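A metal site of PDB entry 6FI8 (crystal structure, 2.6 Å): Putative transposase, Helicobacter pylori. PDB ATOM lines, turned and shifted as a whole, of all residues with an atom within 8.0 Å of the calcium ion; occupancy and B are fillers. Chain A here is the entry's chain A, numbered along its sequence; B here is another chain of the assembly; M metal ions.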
ATOM      1  N   LEU A 125      21.209  -1.213   1.902  1.00  0.00           N
ATOM      2  CA  LEU A 125      21.339   0.030   2.646  1.00  0.00           C
ATOM      3  C   LEU A 125      19.971   0.632   2.996  1.00  0.00           C
ATOM      4  O   LEU A 125      19.822   1.228   4.066  1.00  0.00           O
ATOM      5  CB  LEU A 125      22.168   1.035   1.847  1.00  0.00           C
ATOM      6  CG  LEU A 125      22.425   2.402   2.480  1.00  0.00           C
ATOM      7  CD1 LEU A 125      23.134   2.259   3.829  1.00  0.00           C
ATOM      8  CD2 LEU A 125      23.240   3.280   1.542  1.00  0.00           C
ATOM      9  N   ASN A 126      18.984   0.483   2.114  1.00  0.00           N
ATOM     10  CA  ASN A 126      17.672   1.048   2.403  1.00  0.00           C
ATOM     11  C   ASN A 126      16.977   0.324   3.553  1.00  0.00           C
ATOM     12  O   ASN A 126      16.140   0.916   4.238  1.00  0.00           O
ATOM     13  CB  ASN A 126      16.786   1.015   1.161  1.00  0.00           C
ATOM     14  CG  ASN A 126      16.445  -0.393   0.726  1.00  0.00           C
ATOM     15  OD1 ASN A 126      17.322  -1.243   0.577  1.00  0.00           O
ATOM     16  ND2 ASN A 126      15.160  -0.657   0.529  1.00  0.00           N
ATOM     17  N   VAL A 127      17.318  -0.941   3.771  1.00  0.00           N
ATOM     18  CA  VAL A 127      16.735  -1.697   4.884  1.00  0.00           C
ATOM     19  C   VAL A 127      17.428  -1.353   6.193  1.00  0.00           C
ATOM     20  O   VAL A 127      16.775  -1.195   7.227  1.00  0.00           O
ATOM     21  CB  VAL A 127      16.785  -3.202   4.586  1.00  0.00           C
ATOM     22  CG1 VAL A 127      16.437  -4.006   5.830  1.00  0.00           C
ATOM     23  CG2 VAL A 127      15.837  -3.556   3.443  1.00  0.00           C
ATOM     24  N   VAL A 128      18.758  -1.223   6.162  1.00  0.00           N
ATOM     25  CA  VAL A 128      19.500  -0.949   7.399  1.00  0.00           C
ATOM     26  C   VAL A 128      19.203   0.460   7.911  1.00  0.00           C
ATOM     27  O   VAL A 128      19.179   0.677   9.126  1.00  0.00           O
ATOM     28  CB  VAL A 128      21.004  -1.174   7.161  1.00  0.00           C
ATOM     29  CG1 VAL A 128      21.790  -0.918   8.441  1.00  0.00           C
ATOM     30  CG2 VAL A 128      21.260  -2.578   6.658  1.00  0.00           C
ATOM     31  N   LYS A 129      18.959   1.418   7.014  1.00  0.00           N
ATOM     32  CA  LYS A 129      18.560   2.744   7.461  1.00  0.00           C
ATOM     33  C   LYS A 129      17.231   2.717   8.218  1.00  0.00           C
ATOM     34  O   LYS A 129      16.976   3.605   9.028  1.00  0.00           O
ATOM     35  CB  LYS A 129      18.474   3.716   6.283  1.00  0.00           C
ATOM     36  CG  LYS A 129      19.820   4.272   5.860  1.00  0.00           C
ATOM     37  CD  LYS A 129      19.688   5.449   4.908  1.00  0.00           C
ATOM     38  CE  LYS A 129      20.273   5.113   3.550  1.00  0.00           C
ATOM     39  NZ  LYS A 129      20.774   6.316   2.817  1.00  0.00           N
ATOM     40  N   GLN A 130      16.383   1.709   7.969  1.00  0.00           N
ATOM     41  CA  GLN A 130      15.162   1.563   8.739  1.00  0.00           C
ATOM     42  C   GLN A 130      15.422   1.121  10.170  1.00  0.00           C
ATOM     43  O   GLN A 130      14.584   1.359  11.046  1.00  0.00           O
ATOM     44  CB  GLN A 130      14.219   0.575   8.050  1.00  0.00           C
ATOM     45  CG  GLN A 130      13.816   0.974   6.654  1.00  0.00           C
ATOM     46  CD  GLN A 130      12.963  -0.069   5.967  1.00  0.00           C
ATOM     47  OE1 GLN A 130      12.563  -1.051   6.593  1.00  0.00           O
ATOM     48  NE2 GLN A 130      12.689   0.137   4.688  1.00  0.00           N
ATOM     49  N   TYR A 131      16.571   0.479  10.432  1.00  0.00           N
ATOM     50  CA  TYR A 131      16.903   0.092  11.797  1.00  0.00           C
ATOM     51  C   TYR A 131      17.085   1.313  12.689  1.00  0.00           C
ATOM     52  O   TYR A 131      16.890   1.225  13.903  1.00  0.00           O
ATOM     53  CB  TYR A 131      18.195  -0.737  11.837  1.00  0.00           C
ATOM     54  CG  TYR A 131      18.188  -2.020  11.042  1.00  0.00           C
ATOM     55  CD1 TYR A 131      17.003  -2.606  10.619  1.00  0.00           C
ATOM     56  CD2 TYR A 131      19.382  -2.654  10.710  1.00  0.00           C
ATOM     57  CE1 TYR A 131      17.001  -3.781   9.898  1.00  0.00           C
ATOM     58  CE2 TYR A 131      19.389  -3.825   9.993  1.00  0.00           C
ATOM     59  CZ  TYR A 131      18.201  -4.391   9.583  1.00  0.00           C
ATOM     60  OH  TYR A 131      18.222  -5.564   8.863  1.00  0.00           O
ATOM     61  N   ILE A 132      17.466   2.444  12.109  1.00  0.00           N
ATOM     62  CA  ILE A 132      17.893   3.622  12.845  1.00  0.00           C
ATOM     63  C   ILE A 132      16.931   4.766  12.572  1.00  0.00           C
ATOM     64  O   ILE A 132      16.668   5.099  11.414  1.00  0.00           O
ATOM     65  CB  ILE A 132      19.325   4.023  12.456  1.00  0.00           C
ATOM     66  CG1 ILE A 132      20.281   2.841  12.653  1.00  0.00           C
ATOM     67  CG2 ILE A 132      19.783   5.229  13.252  1.00  0.00           C
ATOM     68  CD1 ILE A 132      21.630   3.039  12.012  1.00  0.00           C
ATOM     69  N   GLU A 133      16.405   5.360  13.645  1.00  0.00           N
ATOM     70  CA  GLU A 133      15.634   6.595  13.536  1.00  0.00           C
ATOM     71  C   GLU A 133      16.617   7.756  13.662  1.00  0.00           C
ATOM     72  O   GLU A 133      17.032   8.118  14.759  1.00  0.00           O
ATOM     73  CB  GLU A 133      14.546   6.667  14.611  1.00  0.00           C
ATOM     74  CG  GLU A 133      13.229   6.012  14.219  1.00  0.00           C
ATOM     75  CD  GLU A 133      13.385   4.559  13.813  1.00  0.00           C
ATOM     76  OE1 GLU A 133      13.432   4.273  12.601  1.00  0.00           O
ATOM     77  OE2 GLU A 133      13.473   3.695  14.718  1.00  0.00           O
ATOM     78  N   ASN A 134      16.991   8.325  12.514  1.00  0.00           N
ATOM     79  CA  ASN A 134      18.073   9.303  12.480  1.00  0.00           C
ATOM     80  C   ASN A 134      17.723  10.546  13.292  1.00  0.00           C
ATOM     81  O   ASN A 134      16.654  11.140  13.116  1.00  0.00           O
ATOM     82  CB  ASN A 134      18.395   9.703  11.041  1.00  0.00           C
ATOM     83  CG  ASN A 134      19.607  10.607  10.940  1.00  0.00           C
ATOM     84  OD1 ASN A 134      20.392  10.723  11.877  1.00  0.00           O
ATOM     85  ND2 ASN A 134      19.770  11.248   9.788  1.00  0.00           N
ATOM     86  N   GLN A 135      18.620  10.918  14.192  1.00  0.00           N
ATOM     87  CA  GLN A 135      18.520  12.160  14.950  1.00  0.00           C
ATOM     88  C   GLN A 135      19.491  13.218  14.441  1.00  0.00           C
ATOM     89  O   GLN A 135      19.520  14.327  14.988  1.00  0.00           O
ATOM     90  CB  GLN A 135      18.765  11.874  16.439  1.00  0.00           C
ATOM     91  CG  GLN A 135      17.852  10.781  16.998  1.00  0.00           C
ATOM     92  CD  GLN A 135      18.269  10.327  18.384  1.00  0.00           C
ATOM     93  OE1 GLN A 135      19.384  10.583  18.836  1.00  0.00           O
ATOM     94  NE2 GLN A 135      17.373   9.627  19.070  1.00  0.00           N
ATOM     95  N   ILE B  60      25.925   9.313   8.269  1.00  0.00           N
ATOM     96  CA  ILE B  60      24.667   9.189   7.534  1.00  0.00           C
ATOM     97  C   ILE B  60      23.487   9.253   8.493  1.00  0.00           C
ATOM     98  O   ILE B  60      22.552  10.039   8.309  1.00  0.00           O
ATOM     99  CB  ILE B  60      24.667   7.906   6.701  1.00  0.00           C
ATOM    100  CG1 ILE B  60      25.798   7.948   5.669  1.00  0.00           C
ATOM    101  CG2 ILE B  60      23.319   7.696   6.023  1.00  0.00           C
ATOM    102  CD1 ILE B  60      26.231   6.591   5.154  1.00  0.00           C
ATOM    103  N   GLU B  61      23.507   8.426   9.533  1.00  0.00           N
ATOM    104  CA  GLU B  61      22.483   8.447  10.563  1.00  0.00           C
ATOM    105  C   GLU B  61      23.119   8.147  11.914  1.00  0.00           C
ATOM    106  O   GLU B  61      24.055   7.351  12.008  1.00  0.00           O
ATOM    107  CB  GLU B  61      21.353   7.436  10.292  1.00  0.00           C
ATOM    108  CG  GLU B  61      20.576   7.705   9.011  1.00  0.00           C
ATOM    109  CD  GLU B  61      19.306   6.882   8.908  1.00  0.00           C
ATOM    110  OE1 GLU B  61      18.851   6.377   9.958  1.00  0.00           O
ATOM    111  OE2 GLU B  61      18.772   6.734   7.799  1.00  0.00           O
ATOM    112  N   MET B  62      22.591   8.784  12.960  1.00  0.00           N
ATOM    113  CA  MET B  62      23.042   8.557  14.325  1.00  0.00           C
ATOM    114  C   MET B  62      21.843   8.648  15.254  1.00  0.00           C
ATOM    115  O   MET B  62      21.056   9.600  15.171  1.00  0.00           O
ATOM    116  CB  MET B  62      24.114   9.570  14.733  1.00  0.00           C
ATOM    117  CG  MET B  62      24.571   9.444  16.178  1.00  0.00           C
ATOM    118  SD  MET B  62      26.071  10.372  16.519  1.00  0.00           S
ATOM    119  CE  MET B  62      25.627  11.990  15.896  1.00  0.00           C
ATOM    120  N   GLN B  63      21.709   7.661  16.130  1.00  0.00           N
ATOM    121  CA  GLN B  63      20.615   7.637  17.096  1.00  0.00           C
ATOM    122  C   GLN B  63      21.102   7.029  18.407  1.00  0.00           C
ATOM    123  O   GLN B  63      21.722   5.969  18.409  1.00  0.00           O
ATOM    124  CB  GLN B  63      19.422   6.819  16.576  1.00  0.00           C
ATOM    125  CG  GLN B  63      18.275   6.714  17.568  1.00  0.00           C
ATOM    126  CD  GLN B  63      17.244   5.671  17.168  1.00  0.00           C
ATOM    127  OE1 GLN B  63      17.406   4.970  16.173  1.00  0.00           O
ATOM    128  NE2 GLN B  63      16.176   5.575  17.948  1.00  0.00           N
ATOM    129  N   LEU B  72      25.378   5.021  11.595  1.00  0.00           N
ATOM    130  CA  LEU B  72      25.610   4.630  10.209  1.00  0.00           C
ATOM    131  C   LEU B  72      26.543   5.669   9.602  1.00  0.00           C
ATOM    132  O   LEU B  72      26.181   6.848   9.491  1.00  0.00           O
ATOM    133  CB  LEU B  72      24.303   4.536   9.433  1.00  0.00           C
ATOM    134  CG  LEU B  72      24.434   4.104   7.973  1.00  0.00           C
ATOM    135  CD1 LEU B  72      25.211   2.807   7.877  1.00  0.00           C
ATOM    136  CD2 LEU B  72      23.065   3.957   7.337  1.00  0.00           C
HETATM  137 CA    CA M   1      16.362   5.934   9.195  1.00  0.00          CA
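The calcium ion is bound by the backbone carbonyl oxygen (O) of Ile 132 (2.4 Å), the backbone carbonyl oxygen (O) of Lys 129 (2.4 Å), the side-chain carboxylate (OE1) of Glu 61 of chain B (2.6 Å) and the side-chain carboxylate (OE2) of Glu 61 of chain B (2.9 Å).
The calcium ion has four donor atoms within binding distance.
The backbone carbonyl oxygen of Glu 61 of chain B is in hydrogen-bond range of the backbone NH of Leu 72 of chain B.
Of the 16 residues printed, 3 come within 4 Å of the calcium ion.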
